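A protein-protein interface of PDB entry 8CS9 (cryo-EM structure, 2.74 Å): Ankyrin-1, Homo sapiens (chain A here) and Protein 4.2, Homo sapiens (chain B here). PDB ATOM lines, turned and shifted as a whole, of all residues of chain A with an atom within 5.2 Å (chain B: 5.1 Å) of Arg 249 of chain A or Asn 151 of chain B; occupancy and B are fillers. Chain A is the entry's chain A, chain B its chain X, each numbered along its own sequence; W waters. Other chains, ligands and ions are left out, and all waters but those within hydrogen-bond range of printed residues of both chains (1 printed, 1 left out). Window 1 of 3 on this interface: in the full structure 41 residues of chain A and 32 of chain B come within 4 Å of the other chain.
OE1 of Glu 217 of chain A lies within hydrogen-bond range of N of Glu 152 of chain B. OE2 of Glu 217 of chain A sits close to OD1 of Asn 151 of chain B. The side-chain amide nitrogen (ND2) of Asn 151 of chain B sits at hydrogen-bond distance from the backbone carbonyl oxygen (O) of Gly 250 of chain A, 2.7 Å away.
NE2 of His 284 of chain A is in hydrogen-bond range of N of Gly 250 of chain A, at 3.3 Å. N of Asn 251 of chain A is in hydrogen-bond range of O of Ala 246 of chain A, 3.0 Å away. The backbone carbonyl oxygen of His 215 of chain A lies within hydrogen-bond range of the side-chain amide nitrogen of Asn 251 of chain A (3.4 Å). The guanidinium group of Arg 249 of chain A is in hydrogen-bond range of the backbone carbonyl oxygen of His 215 of chain A (3.0 Å). OE1 of Glu 152 of chain B lies within salt-bridge range of NH2 of Arg 155 of chain B (2.8 Å).
Among the printed residues, pairs that only touch across the chains: Asn 251 of chain A with Asn 151 of chain B (3.5 Å), Glu 217 of chain A with Lys 150 of chain B (3.5 Å), Val 252 of chain A with Ala 153 of chain B (3.7 Å), Arg 249 of chain A with Asn 151 of chain B (3.7 Å), Arg 249 of chain A with Lys 150 of chain B (3.7 Å) and Val 252 of chain A with Asn 151 of chain B (3.8 Å).
Of chain B, only Lys 150 and Asn 151 come within 4 Å of Arg 249 of chain A. Of the printed residues of chain B, Asn 251 of chain A touches Asn 151. Of the printed residues of chain A, Glu 152 of chain B touches Glu 217 (2.8 Å). His 215 of chain A touches none of the printed residues of chain B. The nearest printed residue of chain A that does not touch Asn 151 of chain B is His 284 of chain A (5.9 Å). The nearest printed residue of chain B that does not touch Asn 251 of chain A is Lys 150 of chain B (5.2 Å).
Of the 7 printed residues of chain B, 4 touch a printed residue of chain A. Along chain B the printed residues that touch a printed residue of chain A span positions 150 to 153. Of the 14 printed residues of chain A, 5 touch a printed residue of chain B. Among the printed residues, no Asp or Glu carboxylate lies within 4 Å of a Lys or Arg side-chain nitrogen of the other chain.
Water W1 bridges NH2 of Arg 155 of chain B and OE1 of Glu 217 of chain A.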
ATOM      1  N   ALA A 214     -26.606 -13.733   7.383  1.00  0.00           N
ATOM      2  CA  ALA A 214     -25.329 -13.852   6.692  1.00  0.00           C
ATOM      3  C   ALA A 214     -24.637 -15.169   7.013  1.00  0.00           C
ATOM      4  O   ALA A 214     -23.947 -15.727   6.154  1.00  0.00           O
ATOM      5  CB  ALA A 214     -24.425 -12.676   7.052  1.00  0.00           C
ATOM      6  N   HIS A 215     -24.799 -15.674   8.237  1.00  0.00           N
ATOM      7  CA  HIS A 215     -24.183 -16.947   8.593  1.00  0.00           C
ATOM      8  C   HIS A 215     -24.802 -18.102   7.820  1.00  0.00           C
ATOM      9  O   HIS A 215     -24.084 -18.979   7.329  1.00  0.00           O
ATOM     10  CB  HIS A 215     -24.295 -17.184  10.098  1.00  0.00           C
ATOM     11  CG  HIS A 215     -23.789 -18.523  10.537  1.00  0.00           C
ATOM     12  ND1 HIS A 215     -22.512 -18.713  11.019  1.00  0.00           N
ATOM     13  CD2 HIS A 215     -24.390 -19.735  10.575  1.00  0.00           C
ATOM     14  CE1 HIS A 215     -22.347 -19.986  11.328  1.00  0.00           C
ATOM     15  NE2 HIS A 215     -23.470 -20.627  11.068  1.00  0.00           N
ATOM     16  N   TYR A 216     -26.127 -18.125   7.701  1.00  0.00           N
ATOM     17  CA  TYR A 216     -26.804 -19.231   7.037  1.00  0.00           C
ATOM     18  C   TYR A 216     -27.129 -18.948   5.576  1.00  0.00           C
ATOM     19  O   TYR A 216     -27.743 -19.796   4.921  1.00  0.00           O
ATOM     20  CB  TYR A 216     -28.077 -19.599   7.801  1.00  0.00           C
ATOM     21  CG  TYR A 216     -27.792 -20.293   9.108  1.00  0.00           C
ATOM     22  CD1 TYR A 216     -27.371 -21.616   9.135  1.00  0.00           C
ATOM     23  CD2 TYR A 216     -27.927 -19.625  10.317  1.00  0.00           C
ATOM     24  CE1 TYR A 216     -27.101 -22.253  10.325  1.00  0.00           C
ATOM     25  CE2 TYR A 216     -27.657 -20.255  11.512  1.00  0.00           C
ATOM     26  CZ  TYR A 216     -27.246 -21.569  11.512  1.00  0.00           C
ATOM     27  OH  TYR A 216     -26.977 -22.204  12.701  1.00  0.00           O
ATOM     28  N   GLU A 217     -26.707 -17.799   5.052  1.00  0.00           N
ATOM     29  CA  GLU A 217     -26.997 -17.370   3.682  1.00  0.00           C
ATOM     30  C   GLU A 217     -28.490 -17.455   3.373  1.00  0.00           C
ATOM     31  O   GLU A 217     -28.918 -18.046   2.380  1.00  0.00           O
ATOM     32  CB  GLU A 217     -26.179 -18.150   2.656  1.00  0.00           C
ATOM     33  CG  GLU A 217     -25.819 -17.308   1.440  1.00  0.00           C
ATOM     34  CD  GLU A 217     -25.250 -18.124   0.302  1.00  0.00           C
ATOM     35  OE1 GLU A 217     -25.589 -19.321   0.197  1.00  0.00           O
ATOM     36  OE2 GLU A 217     -24.461 -17.568  -0.487  1.00  0.00           O
ATOM     37  N   HIS A 244     -18.095  -9.879   7.557  1.00  0.00           N
ATOM     38  CA  HIS A 244     -17.102 -10.800   8.106  1.00  0.00           C
ATOM     39  C   HIS A 244     -17.633 -12.225   8.135  1.00  0.00           C
ATOM     40  O   HIS A 244     -16.941 -13.168   7.738  1.00  0.00           O
ATOM     41  CB  HIS A 244     -16.703 -10.367   9.516  1.00  0.00           C
ATOM     42  CG  HIS A 244     -15.694  -9.266   9.556  1.00  0.00           C
ATOM     43  ND1 HIS A 244     -16.039  -7.951   9.777  1.00  0.00           N
ATOM     44  CD2 HIS A 244     -14.348  -9.284   9.423  1.00  0.00           C
ATOM     45  CE1 HIS A 244     -14.951  -7.205   9.768  1.00  0.00           C
ATOM     46  NE2 HIS A 244     -13.910  -7.990   9.557  1.00  0.00           N
ATOM     47  N   ILE A 245     -18.872 -12.397   8.600  1.00  0.00           N
ATOM     48  CA  ILE A 245     -19.451 -13.730   8.707  1.00  0.00           C
ATOM     49  C   ILE A 245     -19.677 -14.330   7.326  1.00  0.00           C
ATOM     50  O   ILE A 245     -19.404 -15.514   7.096  1.00  0.00           O
ATOM     51  CB  ILE A 245     -20.753 -13.685   9.523  1.00  0.00           C
ATOM     52  CG1 ILE A 245     -20.482 -13.167  10.932  1.00  0.00           C
ATOM     53  CG2 ILE A 245     -21.351 -15.055   9.621  1.00  0.00           C
ATOM     54  CD1 ILE A 245     -21.724 -13.016  11.773  1.00  0.00           C
ATOM     55  N   ALA A 246     -20.177 -13.526   6.385  1.00  0.00           N
ATOM     56  CA  ALA A 246     -20.420 -14.027   5.038  1.00  0.00           C
ATOM     57  C   ALA A 246     -19.118 -14.417   4.346  1.00  0.00           C
ATOM     58  O   ALA A 246     -19.076 -15.402   3.601  1.00  0.00           O
ATOM     59  CB  ALA A 246     -21.180 -12.981   4.223  1.00  0.00           C
ATOM     60  N   SER A 247     -18.045 -13.657   4.578  1.00  0.00           N
ATOM     61  CA  SER A 247     -16.756 -14.003   3.990  1.00  0.00           C
ATOM     62  C   SER A 247     -16.158 -15.245   4.643  1.00  0.00           C
ATOM     63  O   SER A 247     -15.551 -16.076   3.962  1.00  0.00           O
ATOM     64  CB  SER A 247     -15.795 -12.821   4.101  1.00  0.00           C
ATOM     65  OG  SER A 247     -16.478 -11.596   3.919  1.00  0.00           O
ATOM     66  N   ARG A 248     -16.313 -15.383   5.961  1.00  0.00           N
ATOM     67  CA  ARG A 248     -15.786 -16.556   6.651  1.00  0.00           C
ATOM     68  C   ARG A 248     -16.531 -17.823   6.249  1.00  0.00           C
ATOM     69  O   ARG A 248     -15.921 -18.888   6.102  1.00  0.00           O
ATOM     70  CB  ARG A 248     -15.862 -16.345   8.162  1.00  0.00           C
ATOM     71  CG  ARG A 248     -14.787 -17.057   8.957  1.00  0.00           C
ATOM     72  CD  ARG A 248     -15.261 -18.422   9.419  1.00  0.00           C
ATOM     73  NE  ARG A 248     -16.496 -18.339  10.187  1.00  0.00           N
ATOM     74  CZ  ARG A 248     -17.097 -19.377  10.751  1.00  0.00           C
ATOM     75  NH1 ARG A 248     -16.614 -20.602  10.635  1.00  0.00           N
ATOM     76  NH2 ARG A 248     -18.214 -19.181  11.446  1.00  0.00           N
ATOM     77  N   ARG A 249     -17.849 -17.732   6.071  1.00  0.00           N
ATOM     78  CA  ARG A 249     -18.661 -18.903   5.778  1.00  0.00           C
ATOM     79  C   ARG A 249     -18.631 -19.308   4.311  1.00  0.00           C
ATOM     80  O   ARG A 249     -19.075 -20.413   3.987  1.00  0.00           O
ATOM     81  CB  ARG A 249     -20.109 -18.657   6.209  1.00  0.00           C
ATOM     82  CG  ARG A 249     -20.309 -18.602   7.715  1.00  0.00           C
ATOM     83  CD  ARG A 249     -20.466 -19.991   8.300  1.00  0.00           C
ATOM     84  NE  ARG A 249     -21.689 -20.635   7.839  1.00  0.00           N
ATOM     85  CZ  ARG A 249     -22.015 -21.894   8.090  1.00  0.00           C
ATOM     86  NH1 ARG A 249     -21.231 -22.681   8.805  1.00  0.00           N
ATOM     87  NH2 ARG A 249     -23.160 -22.373   7.618  1.00  0.00           N
ATOM     88  N   GLY A 250     -18.119 -18.460   3.425  1.00  0.00           N
ATOM     89  CA  GLY A 250     -18.118 -18.778   2.013  1.00  0.00           C
ATOM     90  C   GLY A 250     -19.386 -18.414   1.282  1.00  0.00           C
ATOM     91  O   GLY A 250     -19.644 -18.956   0.205  1.00  0.00           O
ATOM     92  N   ASN A 251     -20.184 -17.501   1.830  1.00  0.00           N
ATOM     93  CA  ASN A 251     -21.464 -17.115   1.243  1.00  0.00           C
ATOM     94  C   ASN A 251     -21.207 -16.049   0.189  1.00  0.00           C
ATOM     95  O   ASN A 251     -21.192 -14.853   0.475  1.00  0.00           O
ATOM     96  CB  ASN A 251     -22.415 -16.625   2.325  1.00  0.00           C
ATOM     97  CG  ASN A 251     -22.725 -17.691   3.351  1.00  0.00           C
ATOM     98  OD1 ASN A 251     -22.525 -18.877   3.106  1.00  0.00           O
ATOM     99  ND2 ASN A 251     -23.206 -17.271   4.511  1.00  0.00           N
ATOM    100  N   VAL A 252     -21.005 -16.497  -1.051  1.00  0.00           N
ATOM    101  CA  VAL A 252     -20.682 -15.586  -2.145  1.00  0.00           C
ATOM    102  C   VAL A 252     -21.846 -14.643  -2.423  1.00  0.00           C
ATOM    103  O   VAL A 252     -21.661 -13.430  -2.589  1.00  0.00           O
ATOM    104  CB  VAL A 252     -20.296 -16.389  -3.400  1.00  0.00           C
ATOM    105  CG1 VAL A 252     -19.891 -15.463  -4.525  1.00  0.00           C
ATOM    106  CG2 VAL A 252     -19.185 -17.367  -3.077  1.00  0.00           C
ATOM    107  N   HIS A 284     -11.569 -19.158   0.404  1.00  0.00           N
ATOM    108  CA  HIS A 284     -12.668 -18.841  -0.505  1.00  0.00           C
ATOM    109  C   HIS A 284     -12.115 -17.926  -1.593  1.00  0.00           C
ATOM    110  O   HIS A 284     -11.965 -16.721  -1.402  1.00  0.00           O
ATOM    111  CB  HIS A 284     -13.824 -18.208   0.257  1.00  0.00           C
ATOM    112  CG  HIS A 284     -14.413 -19.106   1.297  1.00  0.00           C
ATOM    113  ND1 HIS A 284     -14.785 -20.404   1.032  1.00  0.00           N
ATOM    114  CD2 HIS A 284     -14.676 -18.900   2.609  1.00  0.00           C
ATOM    115  CE1 HIS A 284     -15.262 -20.957   2.132  1.00  0.00           C
ATOM    116  NE2 HIS A 284     -15.206 -20.066   3.104  1.00  0.00           N
ATOM    117  N   LEU B 149     -27.458 -28.312   0.284  1.00  0.00           N
ATOM    118  CA  LEU B 149     -26.184 -27.612   0.222  1.00  0.00           C
ATOM    119  C   LEU B 149     -26.342 -26.244   0.869  1.00  0.00           C
ATOM    120  O   LEU B 149     -27.295 -25.519   0.566  1.00  0.00           O
ATOM    121  CB  LEU B 149     -25.702 -27.468  -1.222  1.00  0.00           C
ATOM    122  CG  LEU B 149     -24.736 -28.513  -1.777  1.00  0.00           C
ATOM    123  CD1 LEU B 149     -24.436 -28.235  -3.237  1.00  0.00           C
ATOM    124  CD2 LEU B 149     -23.456 -28.552  -0.966  1.00  0.00           C
ATOM    125  N   LYS B 150     -25.408 -25.899   1.758  1.00  0.00           N
ATOM    126  CA  LYS B 150     -25.500 -24.645   2.500  1.00  0.00           C
ATOM    127  C   LYS B 150     -25.388 -23.435   1.581  1.00  0.00           C
ATOM    128  O   LYS B 150     -26.100 -22.442   1.758  1.00  0.00           O
ATOM    129  CB  LYS B 150     -24.409 -24.586   3.568  1.00  0.00           C
ATOM    130  CG  LYS B 150     -24.473 -25.679   4.610  1.00  0.00           C
ATOM    131  CD  LYS B 150     -23.348 -25.523   5.620  1.00  0.00           C
ATOM    132  CE  LYS B 150     -22.668 -26.850   5.908  1.00  0.00           C
ATOM    133  NZ  LYS B 150     -21.797 -27.291   4.784  1.00  0.00           N
ATOM    134  N   ASN B 151     -24.495 -23.498   0.601  1.00  0.00           N
ATOM    135  CA  ASN B 151     -24.120 -22.345  -0.200  1.00  0.00           C
ATOM    136  C   ASN B 151     -24.858 -22.344  -1.531  1.00  0.00           C
ATOM    137  O   ASN B 151     -25.005 -23.386  -2.173  1.00  0.00           O
ATOM    138  CB  ASN B 151     -22.609 -22.341  -0.449  1.00  0.00           C
ATOM    139  CG  ASN B 151     -21.955 -21.054  -0.025  1.00  0.00           C
ATOM    140  OD1 ASN B 151     -22.324 -19.976  -0.487  1.00  0.00           O
ATOM    141  ND2 ASN B 151     -20.980 -21.155   0.867  1.00  0.00           N
ATOM    142  N   GLU B 152     -25.319 -21.161  -1.941  1.00  0.00           N
ATOM    143  CA  GLU B 152     -25.914 -21.026  -3.266  1.00  0.00           C
ATOM    144  C   GLU B 152     -24.858 -21.131  -4.359  1.00  0.00           C
ATOM    145  O   GLU B 152     -25.125 -21.675  -5.436  1.00  0.00           O
ATOM    146  CB  GLU B 152     -26.673 -19.704  -3.370  1.00  0.00           C
ATOM    147  CG  GLU B 152     -27.337 -19.489  -4.719  1.00  0.00           C
ATOM    148  CD  GLU B 152     -28.562 -20.365  -4.908  1.00  0.00           C
ATOM    149  OE1 GLU B 152     -29.336 -20.525  -3.943  1.00  0.00           O
ATOM    150  OE2 GLU B 152     -28.746 -20.899  -6.019  1.00  0.00           O
ATOM    151  N   ALA B 153     -23.655 -20.610  -4.107  1.00  0.00           N
ATOM    152  CA  ALA B 153     -22.573 -20.752  -5.076  1.00  0.00           C
ATOM    153  C   ALA B 153     -22.199 -22.214  -5.272  1.00  0.00           C
ATOM    154  O   ALA B 153     -21.974 -22.660  -6.404  1.00  0.00           O
ATOM    155  CB  ALA B 153     -21.357 -19.942  -4.630  1.00  0.00           C
ATOM    156  N   GLN B 154     -22.138 -22.980  -4.181  1.00  0.00           N
ATOM    157  CA  GLN B 154     -21.866 -24.407  -4.296  1.00  0.00           C
ATOM    158  C   GLN B 154     -23.003 -25.128  -5.007  1.00  0.00           C
ATOM    159  O   GLN B 154     -22.764 -26.059  -5.781  1.00  0.00           O
ATOM    160  CB  GLN B 154     -21.625 -25.011  -2.915  1.00  0.00           C
ATOM    161  CG  GLN B 154     -20.342 -24.550  -2.257  1.00  0.00           C
ATOM    162  CD  GLN B 154     -19.955 -25.410  -1.079  1.00  0.00           C
ATOM    163  OE1 GLN B 154     -20.213 -26.612  -1.062  1.00  0.00           O
ATOM    164  NE2 GLN B 154     -19.335 -24.799  -0.080  1.00  0.00           N
ATOM    165  N   ARG B 155     -24.247 -24.712  -4.754  1.00  0.00           N
ATOM    166  CA  ARG B 155     -25.377 -25.291  -5.472  1.00  0.00           C
ATOM    167  C   ARG B 155     -25.255 -25.054  -6.969  1.00  0.00           C
ATOM    168  O   ARG B 155     -25.395 -25.989  -7.763  1.00  0.00           O
ATOM    169  CB  ARG B 155     -26.689 -24.713  -4.943  1.00  0.00           C
ATOM    170  CG  ARG B 155     -27.139 -25.339  -3.650  1.00  0.00           C
ATOM    171  CD  ARG B 155     -28.528 -24.912  -3.252  1.00  0.00           C
ATOM    172  NE  ARG B 155     -28.586 -23.505  -2.883  1.00  0.00           N
ATOM    173  CZ  ARG B 155     -28.764 -23.062  -1.647  1.00  0.00           C
ATOM    174  NH1 ARG B 155     -28.876 -23.892  -0.625  1.00  0.00           N
ATOM    175  NH2 ARG B 155     -28.830 -21.753  -1.432  1.00  0.00           N
HETATM  176  O   HOH W   1     -28.286 -19.643  -0.015  1.00  0.00           O
